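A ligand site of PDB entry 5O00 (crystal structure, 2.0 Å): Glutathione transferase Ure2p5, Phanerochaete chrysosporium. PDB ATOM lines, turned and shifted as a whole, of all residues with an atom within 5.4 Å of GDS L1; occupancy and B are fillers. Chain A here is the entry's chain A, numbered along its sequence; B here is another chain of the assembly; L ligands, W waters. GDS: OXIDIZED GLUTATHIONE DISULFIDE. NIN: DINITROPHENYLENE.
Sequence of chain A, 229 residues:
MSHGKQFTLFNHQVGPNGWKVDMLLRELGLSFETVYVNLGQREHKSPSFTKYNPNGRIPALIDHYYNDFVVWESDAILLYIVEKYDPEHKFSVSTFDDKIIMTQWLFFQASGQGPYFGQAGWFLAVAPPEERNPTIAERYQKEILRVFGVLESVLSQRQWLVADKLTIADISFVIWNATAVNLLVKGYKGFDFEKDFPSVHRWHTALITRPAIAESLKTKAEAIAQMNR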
ATOM      1  N   HIS A  12     -13.299 -30.880   2.335  1.00  0.00           N
ATOM      2  CA  HIS A  12     -14.425 -30.001   2.634  1.00  0.00           C
ATOM      3  C   HIS A  12     -15.695 -30.628   2.074  1.00  0.00           C
ATOM      4  O   HIS A  12     -15.682 -31.262   1.021  1.00  0.00           O
ATOM      5  CB  HIS A  12     -14.247 -28.589   2.060  1.00  0.00           C
ATOM      6  CG  HIS A  12     -15.264 -27.612   2.544  1.00  0.00           C
ATOM      7  ND1 HIS A  12     -16.321 -27.189   1.770  1.00  0.00           N
ATOM      8  CD2 HIS A  12     -15.409 -26.992   3.736  1.00  0.00           C
ATOM      9  CE1 HIS A  12     -17.061 -26.335   2.458  1.00  0.00           C
ATOM     10  NE2 HIS A  12     -16.527 -26.193   3.653  1.00  0.00           N
ATOM     11  N   GLY A  15     -16.922 -28.094  -1.208  1.00  0.00           N
ATOM     12  CA  GLY A  15     -15.919 -27.906  -2.222  1.00  0.00           C
ATOM     13  C   GLY A  15     -15.618 -29.199  -2.963  1.00  0.00           C
ATOM     14  O   GLY A  15     -15.428 -30.247  -2.340  1.00  0.00           O
ATOM     15  N   PRO A  16     -15.553 -29.153  -4.302  1.00  0.00           N
ATOM     16  CA  PRO A  16     -15.326 -30.411  -5.038  1.00  0.00           C
ATOM     17  C   PRO A  16     -13.934 -30.988  -4.894  1.00  0.00           C
ATOM     18  O   PRO A  16     -13.789 -32.223  -4.896  1.00  0.00           O
ATOM     19  CB  PRO A  16     -15.613 -30.006  -6.498  1.00  0.00           C
ATOM     20  CG  PRO A  16     -16.463 -28.816  -6.403  1.00  0.00           C
ATOM     21  CD  PRO A  16     -15.979 -28.072  -5.205  1.00  0.00           C
ATOM     22  N   ASN A  17     -12.895 -30.155  -4.794  1.00  0.00           N
ATOM     23  CA  ASN A  17     -11.575 -30.591  -5.244  1.00  0.00           C
ATOM     24  C   ASN A  17     -10.998 -31.708  -4.367  1.00  0.00           C
ATOM     25  O   ASN A  17     -10.302 -32.587  -4.876  1.00  0.00           O
ATOM     26  CB  ASN A  17     -10.625 -29.395  -5.280  1.00  0.00           C
ATOM     27  CG  ASN A  17     -10.897 -28.511  -6.467  1.00  0.00           C
ATOM     28  OD1 ASN A  17     -10.879 -28.968  -7.610  1.00  0.00           O
ATOM     29  ND2 ASN A  17     -11.176 -27.244  -6.209  1.00  0.00           N
ATOM     30  N   LYS A  20     -11.695 -35.575  -5.451  1.00  0.00           N
ATOM     31  CA  LYS A  20     -10.798 -36.308  -6.342  1.00  0.00           C
ATOM     32  C   LYS A  20      -9.924 -37.263  -5.551  1.00  0.00           C
ATOM     33  O   LYS A  20      -9.755 -38.429  -5.917  1.00  0.00           O
ATOM     34  CB  LYS A  20      -9.891 -35.346  -7.121  1.00  0.00           C
ATOM     35  CG  LYS A  20     -10.558 -34.238  -7.901  1.00  0.00           C
ATOM     36  CD  LYS A  20      -9.475 -33.413  -8.589  1.00  0.00           C
ATOM     37  CE  LYS A  20      -9.978 -32.083  -9.103  1.00  0.00           C
ATOM     38  NZ  LYS A  20      -8.829 -31.206  -9.448  1.00  0.00           N
ATOM     39  N   LEU A  39     -13.861 -23.536   6.038  1.00  0.00           N
ATOM     40  CA  LEU A  39     -13.478 -22.562   5.021  1.00  0.00           C
ATOM     41  C   LEU A  39     -14.305 -21.289   5.164  1.00  0.00           C
ATOM     42  O   LEU A  39     -14.001 -20.431   5.986  1.00  0.00           O
ATOM     43  CB  LEU A  39     -13.665 -23.167   3.625  1.00  0.00           C
ATOM     44  CG  LEU A  39     -12.894 -24.467   3.329  1.00  0.00           C
ATOM     45  CD1 LEU A  39     -13.190 -24.967   1.914  1.00  0.00           C
ATOM     46  CD2 LEU A  39     -11.409 -24.277   3.538  1.00  0.00           C
ATOM     47  N   GLY A  56      -3.345 -22.000   1.528  1.00  0.00           N
ATOM     48  CA  GLY A  56      -4.528 -21.943   2.369  1.00  0.00           C
ATOM     49  C   GLY A  56      -5.769 -22.508   1.717  1.00  0.00           C
ATOM     50  O   GLY A  56      -6.868 -21.974   1.921  1.00  0.00           O
ATOM     51  N   ARG A  57      -5.623 -23.573   0.942  1.00  0.00           N
ATOM     52  CA  ARG A  57      -6.747 -24.195   0.254  1.00  0.00           C
ATOM     53  C   ARG A  57      -6.703 -25.701   0.470  1.00  0.00           C
ATOM     54  O   ARG A  57      -5.628 -26.299   0.614  1.00  0.00           O
ATOM     55  CB  ARG A  57      -6.723 -23.861  -1.247  1.00  0.00           C
ATOM     56  CG  ARG A  57      -6.747 -22.359  -1.566  1.00  0.00           C
ATOM     57  CD  ARG A  57      -8.077 -21.738  -1.173  1.00  0.00           C
ATOM     58  NE  ARG A  57      -8.242 -20.370  -1.661  1.00  0.00           N
ATOM     59  CZ  ARG A  57      -7.973 -19.276  -0.953  1.00  0.00           C
ATOM     60  NH1 ARG A  57      -8.175 -18.080  -1.493  1.00  0.00           N
ATOM     61  NH2 ARG A  57      -7.519 -19.357   0.299  1.00  0.00           N
ATOM     62  N   ILE A  58      -7.878 -26.321   0.509  1.00  0.00           N
ATOM     63  CA  ILE A  58      -7.961 -27.781   0.545  1.00  0.00           C
ATOM     64  C   ILE A  58      -8.018 -28.257  -0.890  1.00  0.00           C
ATOM     65  O   ILE A  58      -8.472 -27.503  -1.775  1.00  0.00           O
ATOM     66  CB  ILE A  58      -9.169 -28.270   1.371  1.00  0.00           C
ATOM     67  CG1 ILE A  58     -10.485 -27.963   0.643  1.00  0.00           C
ATOM     68  CG2 ILE A  58      -9.183 -27.643   2.749  1.00  0.00           C
ATOM     69  CD1 ILE A  58     -10.996 -29.086  -0.264  1.00  0.00           C
ATOM     70  N   PRO A  59      -7.594 -29.489  -1.199  1.00  0.00           N
ATOM     71  CA  PRO A  59      -7.104 -30.477  -0.241  1.00  0.00           C
ATOM     72  C   PRO A  59      -5.626 -30.347   0.073  1.00  0.00           C
ATOM     73  O   PRO A  59      -4.865 -29.661  -0.617  1.00  0.00           O
ATOM     74  CB  PRO A  59      -7.383 -31.798  -0.949  1.00  0.00           C
ATOM     75  CG  PRO A  59      -7.215 -31.475  -2.392  1.00  0.00           C
ATOM     76  CD  PRO A  59      -7.719 -30.061  -2.554  1.00  0.00           C
ATOM     77  N   GLU A  73      -2.417 -29.272  -3.615  1.00  0.00           N
ATOM     78  CA  GLU A  73      -2.912 -29.319  -4.998  1.00  0.00           C
ATOM     79  C   GLU A  73      -3.469 -30.704  -5.306  1.00  0.00           C
ATOM     80  O   GLU A  73      -2.722 -31.680  -5.382  1.00  0.00           O
ATOM     81  CB  GLU A  73      -1.855 -28.942  -6.040  1.00  0.00           C
ATOM     82  CG  GLU A  73      -1.562 -27.453  -6.130  1.00  0.00           C
ATOM     83  CD  GLU A  73      -2.773 -26.630  -6.519  1.00  0.00           C
ATOM     84  OE1 GLU A  73      -3.573 -27.089  -7.358  1.00  0.00           O
ATOM     85  OE2 GLU A  73      -2.928 -25.512  -5.962  1.00  0.00           O
ATOM     86  N   SER A  74      -4.781 -30.769  -5.522  1.00  0.00           N
ATOM     87  CA  SER A  74      -5.470 -32.051  -5.635  1.00  0.00           C
ATOM     88  C   SER A  74      -4.838 -32.958  -6.682  1.00  0.00           C
ATOM     89  O   SER A  74      -4.685 -34.157  -6.462  1.00  0.00           O
ATOM     90  CB  SER A  74      -6.957 -31.822  -5.958  1.00  0.00           C
ATOM     91  OG  SER A  74      -7.129 -31.026  -7.117  1.00  0.00           O
ATOM     92  N   ASP A  75      -4.457 -32.407  -7.848  1.00  0.00           N
ATOM     93  CA  ASP A  75      -3.928 -33.270  -8.898  1.00  0.00           C
ATOM     94  C   ASP A  75      -2.491 -33.683  -8.617  1.00  0.00           C
ATOM     95  O   ASP A  75      -2.068 -34.758  -9.048  1.00  0.00           O
ATOM     96  CB  ASP A  75      -4.017 -32.575 -10.256  1.00  0.00           C
ATOM     97  CG  ASP A  75      -5.445 -32.503 -10.797  1.00  0.00           C
ATOM     98  OD1 ASP A  75      -6.360 -33.042 -10.137  1.00  0.00           O
ATOM     99  OD2 ASP A  75      -5.641 -31.905 -11.877  1.00  0.00           O
ATOM    100  N   ALA A 110      -6.736 -29.310 -14.235  1.00  0.00           N
ATOM    101  CA  ALA A 110      -6.407 -28.362 -13.185  1.00  0.00           C
ATOM    102  C   ALA A 110      -6.514 -26.923 -13.652  1.00  0.00           C
ATOM    103  O   ALA A 110      -6.857 -26.047 -12.855  1.00  0.00           O
ATOM    104  CB  ALA A 110      -4.991 -28.640 -12.663  1.00  0.00           C
ATOM    105  N   GLY A 114     -11.317 -27.070 -13.484  1.00  0.00           N
ATOM    106  CA  GLY A 114     -11.530 -26.613 -12.127  1.00  0.00           C
ATOM    107  C   GLY A 114     -11.759 -25.123 -12.007  1.00  0.00           C
ATOM    108  O   GLY A 114     -12.773 -24.674 -11.459  1.00  0.00           O
ATOM    109  N   PRO A 115     -10.820 -24.320 -12.498  1.00  0.00           N
ATOM    110  CA  PRO A 115     -10.960 -22.858 -12.336  1.00  0.00           C
ATOM    111  C   PRO A 115     -12.178 -22.271 -13.023  1.00  0.00           C
ATOM    112  O   PRO A 115     -12.864 -21.412 -12.443  1.00  0.00           O
ATOM    113  CB  PRO A 115      -9.653 -22.319 -12.921  1.00  0.00           C
ATOM    114  CG  PRO A 115      -8.677 -23.441 -12.803  1.00  0.00           C
ATOM    115  CD  PRO A 115      -9.493 -24.687 -13.021  1.00  0.00           C
ATOM    116  N   GLY A 118     -15.356 -23.502 -11.511  1.00  0.00           N
ATOM    117  CA  GLY A 118     -15.481 -22.841 -10.221  1.00  0.00           C
ATOM    118  C   GLY A 118     -15.971 -21.407 -10.319  1.00  0.00           C
ATOM    119  O   GLY A 118     -16.683 -20.943  -9.422  1.00  0.00           O
ATOM    120  N   GLN A 119     -15.610 -20.691 -11.391  1.00  0.00           N
ATOM    121  CA  GLN A 119     -16.116 -19.330 -11.559  1.00  0.00           C
ATOM    122  C   GLN A 119     -17.604 -19.347 -11.894  1.00  0.00           C
ATOM    123  O   GLN A 119     -18.351 -18.471 -11.438  1.00  0.00           O
ATOM    124  CB  GLN A 119     -15.353 -18.588 -12.659  1.00  0.00           C
ATOM    125  CG  GLN A 119     -13.874 -18.400 -12.396  1.00  0.00           C
ATOM    126  CD  GLN A 119     -13.563 -18.167 -10.933  1.00  0.00           C
ATOM    127  OE1 GLN A 119     -13.808 -17.078 -10.409  1.00  0.00           O
ATOM    128  NE2 GLN A 119     -13.033 -19.182 -10.268  1.00  0.00           N
ATOM    129  N   TRP A 122     -19.096 -19.894  -8.518  1.00  0.00           N
ATOM    130  CA  TRP A 122     -19.058 -18.662  -7.746  1.00  0.00           C
ATOM    131  C   TRP A 122     -20.212 -17.744  -8.108  1.00  0.00           C
ATOM    132  O   TRP A 122     -21.024 -17.363  -7.262  1.00  0.00           O
ATOM    133  CB  TRP A 122     -17.716 -17.951  -7.947  1.00  0.00           C
ATOM    134  CG  TRP A 122     -17.631 -16.682  -7.191  1.00  0.00           C
ATOM    135  CD1 TRP A 122     -17.752 -15.416  -7.681  1.00  0.00           C
ATOM    136  CD2 TRP A 122     -17.411 -16.551  -5.791  1.00  0.00           C
ATOM    137  NE1 TRP A 122     -17.619 -14.500  -6.667  1.00  0.00           N
ATOM    138  CE2 TRP A 122     -17.408 -15.174  -5.493  1.00  0.00           C
ATOM    139  CE3 TRP A 122     -17.217 -17.469  -4.751  1.00  0.00           C
ATOM    140  CZ2 TRP A 122     -17.219 -14.697  -4.211  1.00  0.00           C
ATOM    141  CZ3 TRP A 122     -17.036 -16.994  -3.481  1.00  0.00           C
ATOM    142  CH2 TRP A 122     -17.040 -15.614  -3.212  1.00  0.00           C
ATOM    143  N   VAL A 126     -22.392 -20.022  -5.225  1.00  0.00           N
ATOM    144  CA  VAL A 126     -21.724 -20.097  -3.925  1.00  0.00           C
ATOM    145  C   VAL A 126     -21.139 -18.768  -3.459  1.00  0.00           C
ATOM    146  O   VAL A 126     -20.772 -18.660  -2.283  1.00  0.00           O
ATOM    147  CB  VAL A 126     -20.639 -21.196  -3.901  1.00  0.00           C
ATOM    148  CG1 VAL A 126     -21.256 -22.552  -4.277  1.00  0.00           C
ATOM    149  CG2 VAL A 126     -19.484 -20.855  -4.813  1.00  0.00           C
ATOM    150  N   TRP A 176     -16.061 -32.229 -10.656  1.00  0.00           N
ATOM    151  CA  TRP A 176     -16.530 -30.988 -11.276  1.00  0.00           C
ATOM    152  C   TRP A 176     -17.513 -31.261 -12.409  1.00  0.00           C
ATOM    153  O   TRP A 176     -18.435 -30.458 -12.617  1.00  0.00           O
ATOM    154  CB  TRP A 176     -15.352 -30.160 -11.788  1.00  0.00           C
ATOM    155  CG  TRP A 176     -14.726 -29.269 -10.739  1.00  0.00           C
ATOM    156  CD1 TRP A 176     -13.467 -29.375 -10.217  1.00  0.00           C
ATOM    157  CD2 TRP A 176     -15.328 -28.135 -10.102  1.00  0.00           C
ATOM    158  NE1 TRP A 176     -13.257 -28.380  -9.293  1.00  0.00           N
ATOM    159  CE2 TRP A 176     -14.377 -27.603  -9.197  1.00  0.00           C
ATOM    160  CE3 TRP A 176     -16.581 -27.517 -10.193  1.00  0.00           C
ATOM    161  CZ2 TRP A 176     -14.648 -26.489  -8.406  1.00  0.00           C
ATOM    162  CZ3 TRP A 176     -16.843 -26.414  -9.405  1.00  0.00           C
ATOM    163  CH2 TRP A 176     -15.883 -25.913  -8.526  1.00  0.00           C
ATOM    164  N   PHE B 107       1.382 -27.246 -10.496  1.00  0.00           N
ATOM    165  CA  PHE B 107      -0.077 -27.275 -10.473  1.00  0.00           C
ATOM    166  C   PHE B 107      -0.653 -26.021  -9.820  1.00  0.00           C
ATOM    167  O   PHE B 107      -1.708 -25.548 -10.239  1.00  0.00           O
ATOM    168  CB  PHE B 107      -0.584 -28.538  -9.768  1.00  0.00           C
ATOM    169  CG  PHE B 107      -0.729 -29.714 -10.702  1.00  0.00           C
ATOM    170  CD1 PHE B 107      -1.763 -29.770 -11.615  1.00  0.00           C
ATOM    171  CD2 PHE B 107       0.194 -30.734 -10.676  1.00  0.00           C
ATOM    172  CE1 PHE B 107      -1.880 -30.845 -12.489  1.00  0.00           C
ATOM    173  CE2 PHE B 107       0.077 -31.813 -11.534  1.00  0.00           C
ATOM    174  CZ  PHE B 107      -0.972 -31.852 -12.448  1.00  0.00           C
ATOM    175  N   SER B 111      -3.214 -23.845 -11.933  1.00  0.00           N
ATOM    176  CA  SER B 111      -4.592 -23.728 -11.473  1.00  0.00           C
ATOM    177  C   SER B 111      -4.849 -22.439 -10.700  1.00  0.00           C
ATOM    178  O   SER B 111      -5.990 -21.949 -10.713  1.00  0.00           O
ATOM    179  CB  SER B 111      -4.967 -24.919 -10.585  1.00  0.00           C
ATOM    180  OG  SER B 111      -4.302 -24.883  -9.342  1.00  0.00           O
ATOM    181  N   GLY B 112      -3.828 -21.877 -10.058  1.00  0.00           N
ATOM    182  CA  GLY B 112      -3.999 -20.744  -9.171  1.00  0.00           C
ATOM    183  C   GLY B 112      -3.494 -19.422  -9.701  1.00  0.00           C
ATOM    184  O   GLY B 112      -4.023 -18.362  -9.328  1.00  0.00           O
ATOM    185  N   TYR B 116      -6.596 -17.261 -12.842  1.00  0.00           N
ATOM    186  CA  TYR B 116      -7.121 -16.096 -12.147  1.00  0.00           C
ATOM    187  C   TYR B 116      -6.471 -14.805 -12.643  1.00  0.00           C
ATOM    188  O   TYR B 116      -7.148 -13.790 -12.797  1.00  0.00           O
ATOM    189  CB  TYR B 116      -6.938 -16.273 -10.652  1.00  0.00           C
ATOM    190  CG  TYR B 116      -7.823 -17.381 -10.105  1.00  0.00           C
ATOM    191  CD1 TYR B 116      -7.400 -18.703 -10.108  1.00  0.00           C
ATOM    192  CD2 TYR B 116      -9.102 -17.097  -9.639  1.00  0.00           C
ATOM    193  CE1 TYR B 116      -8.216 -19.714  -9.641  1.00  0.00           C
ATOM    194  CE2 TYR B 116      -9.924 -18.114  -9.167  1.00  0.00           C
ATOM    195  CZ  TYR B 116      -9.467 -19.421  -9.169  1.00  0.00           C
ATOM    196  OH  TYR B 116     -10.275 -20.443  -8.705  1.00  0.00           O
ATOM    197  N   ARG B 139     -12.267  -8.496  -8.378  1.00  0.00           N
ATOM    198  CA  ARG B 139     -12.231  -9.814  -7.755  1.00  0.00           C
ATOM    199  C   ARG B 139     -10.914 -10.520  -8.061  1.00  0.00           C
ATOM    200  O   ARG B 139     -10.314 -11.158  -7.190  1.00  0.00           O
ATOM    201  CB  ARG B 139     -13.426 -10.652  -8.218  1.00  0.00           C
ATOM    202  CG  ARG B 139     -13.274 -12.174  -8.022  1.00  0.00           C
ATOM    203  CD  ARG B 139     -14.557 -12.944  -8.377  1.00  0.00           C
ATOM    204  NE  ARG B 139     -14.317 -14.387  -8.444  1.00  0.00           N
ATOM    205  CZ  ARG B 139     -14.155 -15.175  -7.372  1.00  0.00           C
ATOM    206  NH1 ARG B 139     -14.205 -14.662  -6.162  1.00  0.00           N
ATOM    207  NH2 ARG B 139     -13.936 -16.474  -7.541  1.00  0.00           N
ATOM    208  N   GLU B 143      -7.283 -11.460  -6.145  1.00  0.00           N
ATOM    209  CA  GLU B 143      -6.710 -12.795  -6.169  1.00  0.00           C
ATOM    210  C   GLU B 143      -5.238 -12.753  -6.577  1.00  0.00           C
ATOM    211  O   GLU B 143      -4.432 -13.546  -6.077  1.00  0.00           O
ATOM    212  CB  GLU B 143      -7.518 -13.691  -7.119  1.00  0.00           C
ATOM    213  CG  GLU B 143      -7.057 -15.140  -7.142  1.00  0.00           C
ATOM    214  CD  GLU B 143      -7.229 -15.854  -5.809  1.00  0.00           C
ATOM    215  OE1 GLU B 143      -7.953 -15.329  -4.938  1.00  0.00           O
ATOM    216  OE2 GLU B 143      -6.646 -16.940  -5.637  1.00  0.00           O
HETATM  217  N1  GDS L   1      -6.221 -26.036  -7.668  1.00  0.00           N
HETATM  218  CA1 GDS L   1      -6.559 -26.280  -6.277  1.00  0.00           C
HETATM  219  C1  GDS L   1      -6.671 -27.782  -6.059  1.00  0.00           C
HETATM  220  OE1 GDS L   1      -7.182 -28.491  -6.957  1.00  0.00           O
HETATM  221  OE2 GDS L   1      -6.263 -28.281  -4.988  1.00  0.00           O
HETATM  222  CB1 GDS L   1      -7.911 -25.661  -5.936  1.00  0.00           C
HETATM  223  CG1 GDS L   1      -8.260 -26.023  -4.495  1.00  0.00           C
HETATM  224  CD1 GDS L   1      -9.490 -25.226  -4.064  1.00  0.00           C
HETATM  225  O1  GDS L   1     -10.008 -24.443  -4.791  1.00  0.00           O
HETATM  226  N2  GDS L   1      -9.993 -25.466  -2.724  1.00  0.00           N
HETATM  227  CA2 GDS L   1     -11.150 -24.758  -2.198  1.00  0.00           C
HETATM  228  C2  GDS L   1     -10.733 -23.964  -0.968  1.00  0.00           C
HETATM  229  O2  GDS L   1      -9.945 -24.412  -0.213  1.00  0.00           O
HETATM  230  CB2 GDS L   1     -12.208 -25.770  -1.770  1.00  0.00           C
HETATM  231  SG2 GDS L   1     -13.007 -26.453  -3.239  1.00  0.00           S
HETATM  232  N3  GDS L   1     -11.320 -22.659  -0.707  1.00  0.00           N
HETATM  233  CA3 GDS L   1     -10.923 -21.901   0.474  1.00  0.00           C
HETATM  234  C3  GDS L   1     -10.932 -20.410   0.140  1.00  0.00           C
HETATM  235  OE3 GDS L   1     -11.162 -20.034  -1.026  1.00  0.00           O
HETATM  236  OE4 GDS L   1     -10.703 -19.567   1.051  1.00  0.00           O
HETATM  237  N4  GDS L   1     -11.685 -23.817  -7.228  1.00  0.00           N
HETATM  238  CA4 GDS L   1     -11.154 -23.655  -8.563  1.00  0.00           C
HETATM  239  C4  GDS L   1     -10.479 -24.953  -8.986  1.00  0.00           C
HETATM  240  OE5 GDS L   1      -9.436 -24.919  -9.676  1.00  0.00           O
HETATM  241  OE6 GDS L   1     -10.969 -26.059  -8.631  1.00  0.00           O
HETATM  242  C5  GDS L   1     -12.879 -23.113  -6.820  1.00  0.00           C
HETATM  243  O5  GDS L   1     -13.457 -22.391  -7.576  1.00  0.00           O
HETATM  244  CA5 GDS L   1     -13.397 -23.329  -5.409  1.00  0.00           C
HETATM  245  N5  GDS L   1     -14.161 -22.176  -5.011  1.00  0.00           N
HETATM  246  CB5 GDS L   1     -14.295 -24.563  -5.390  1.00  0.00           C
HETATM  247  SG5 GDS L   1     -14.547 -25.098  -3.672  1.00  0.00           S
HETATM  248  CA6 GDS L   1     -12.582 -18.643  -3.386  1.00  0.00           C
HETATM  249  C6  GDS L   1     -13.105 -17.713  -4.482  1.00  0.00           C
HETATM  250  OE7 GDS L   1     -13.294 -16.499  -4.251  1.00  0.00           O
HETATM  251  OE8 GDS L   1     -13.348 -18.186  -5.624  1.00  0.00           O
HETATM  252  N6  GDS L   1     -11.720 -17.902  -2.470  1.00  0.00           N
HETATM  253  CB6 GDS L   1     -13.761 -19.232  -2.604  1.00  0.00           C
HETATM  254  CG6 GDS L   1     -14.571 -20.168  -3.479  1.00  0.00           C
HETATM  255  CD6 GDS L   1     -13.746 -21.386  -3.870  1.00  0.00           C
HETATM  256  O6  GDS L   1     -12.779 -21.692  -3.243  1.00  0.00           O
HETATM  257  C1  NIN L   2     -20.501 -24.648  -7.203  1.00  0.00           C
HETATM  258  C2  NIN L   2     -19.622 -25.212  -6.301  1.00  0.00           C
HETATM  259  N2  NIN L   2     -18.354 -24.533  -6.080  1.00  0.00           N
HETATM  260  O21 NIN L   2     -17.964 -23.527  -6.966  1.00  0.00           O
HETATM  261  O22 NIN L   2     -17.660 -24.839  -5.175  1.00  0.00           O
HETATM  262  C3  NIN L   2     -19.953 -26.376  -5.633  1.00  0.00           C
HETATM  263  C4  NIN L   2     -21.186 -26.962  -5.881  1.00  0.00           C
HETATM  264  N4  NIN L   2     -21.598 -28.180  -5.223  1.00  0.00           N
HETATM  265  O41 NIN L   2     -20.807 -28.771  -4.223  1.00  0.00           O
HETATM  266  O42 NIN L   2     -22.605 -28.680  -5.560  1.00  0.00           O
HETATM  267  C5  NIN L   2     -22.064 -26.404  -6.790  1.00  0.00           C
HETATM  268  C6  NIN L   2     -21.719 -25.232  -7.451  1.00  0.00           C
HETATM  269  O   HOH W   1      -4.770 -27.741  -2.665  1.00  0.00           O
HETATM  270  O   HOH W   2      -9.367 -18.392  -4.611  1.00  0.00           O
HETATM  271  O   HOH W   3      -4.420 -29.541  -8.664  1.00  0.00           O
HETATM  272  O   HOH W   4      -9.780 -28.608 -10.018  1.00  0.00           O
HETATM  273  O   HOH W   5     -12.779 -19.709  -7.558  1.00  0.00           O
HETATM  274  O   HOH W   6      -4.588 -23.682  -6.938  1.00  0.00           O
HETATM  275  O   HOH W   7      -7.545 -23.491  -8.373  1.00  0.00           O
HETATM  276  O   HOH W   8     -16.358 -21.510  -6.540  1.00  0.00           O
HETATM  277  O   HOH W   9      -7.807 -26.715 -10.288  1.00  0.00           O
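The side-chain hydroxyl of Ser 74 is in hydrogen-bond range of the side-chain amino group of Lys 20 (2.9 Å). The guanidinium group (NH2) of Arg 139 of chain B lies within hydrogen-bond range of the side-chain amide oxygen (OE1) of Gln 119 (2.9 Å). NE1 of Trp 176 sits at hydrogen-bond distance from OD1 of Asn 17 (3.0 Å). OE1 of Glu 73 sits at hydrogen-bond distance from OG of Ser 111 of chain B (3.1 Å). OG of Ser 111 of chain B sits at hydrogen-bond distance from O of Phe 107 of chain B (2.8 Å). The side-chain amide nitrogen of Gln 119 lies within hydrogen-bond range of the backbone carbonyl oxygen of Pro 115, at 3.1 Å. The side-chain amide nitrogen (NE2) of Gln 119 lies within hydrogen-bond range of the side-chain hydroxyl (OH) of Tyr 116 of chain B, at 3.4 Å. N of Gly 15 sits at hydrogen-bond distance from ND1 of His 12 (3.2 Å).
The backbone nitrogen (N) of Pro 115 sits close to an oxygen (OE5) of GDS L1. Residues that only touch GDS L1: Gly 114, Tyr 116 of chain B, Pro 59, Gly 118, Gly 15, Pro 16, Trp 122 and Leu 39. Hydrophobic or aromatic side chains within 4 Å of GDS L1: Pro 16, Leu 39, Ile 58, Pro 59, Pro 115, Trp 122 and Trp 176. Of the 27 residues printed, 17 come within 4 Å of GDS L1.
Water W9 lies within hydrogen-bond range of an oxygen (OE5) of GDS L1 (2.5 Å) and the backbone carbonyl oxygen of Ala 110 (2.8 Å). Water W5 lies within hydrogen-bond range of OE8 of GDS L1, NE2 of Gln 119, OH of Tyr 116 of chain B and NH2 of Arg 139 of chain B. Water W8 lies within hydrogen-bond range of O21 of NIN L2 (2.6 Å), N5 of GDS L1 (2.8 Å) and O of Gly 118 (3.0 Å). Water W6 lies within hydrogen-bond range of OE2 of Glu 73 (2.7 Å), OG of Ser 111 of chain B (2.7 Å) and N1 of GDS L1 (3.0 Å). Water W2 lies within hydrogen-bond range of N6 of GDS L1 (3.2 Å), OE2 of Glu 143 of chain B (3.3 Å) and NH1 of Arg 57 (3.4 Å). Water W3 lies within hydrogen-bond range of OE1 of Glu 73 (2.9 Å), N of Asp 75 (3.0 Å), N of Ser 74 (3.4 Å) and OE1 of GDS L1 (3.4 Å).
The backbone NH of Ser 74 sits at hydrogen-bond distance from an oxygen (OE2) of GDS L1 (2.9 Å). An oxygen (OE1) of GDS L1 lies within hydrogen-bond range of the side-chain hydroxyl of Ser 74, 2.5 Å away. An oxygen (OE8) of GDS L1 lies within salt-bridge range of the guanidinium group of Arg 139 of chain B (2.6 Å). An oxygen (OE6) of GDS L1 lies within hydrogen-bond range of the side-chain amide nitrogen (ND2) of Asn 17, at 2.7 Å. O2 of GDS L1 is in hydrogen-bond range of N of Ile 58 (2.9 Å). The backbone carbonyl oxygen (O) of Ile 58 lies within hydrogen-bond range of a nitrogen (N2) of GDS L1. A nitrogen (N1) of GDS L1 lies within hydrogen-bond range of the side-chain hydroxyl (OG) of Ser 111 of chain B, at 2.8 Å. The side-chain carboxylate (OE1) of Glu 73 is in salt-bridge range of a nitrogen (N1) of GDS L1 (2.9 Å). NE of Arg 57 lies within salt-bridge range of OE3 of GDS L1 (3.0 Å). NE1 of Trp 176 sits at hydrogen-bond distance from OE6 of GDS L1, at 3.3 Å.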
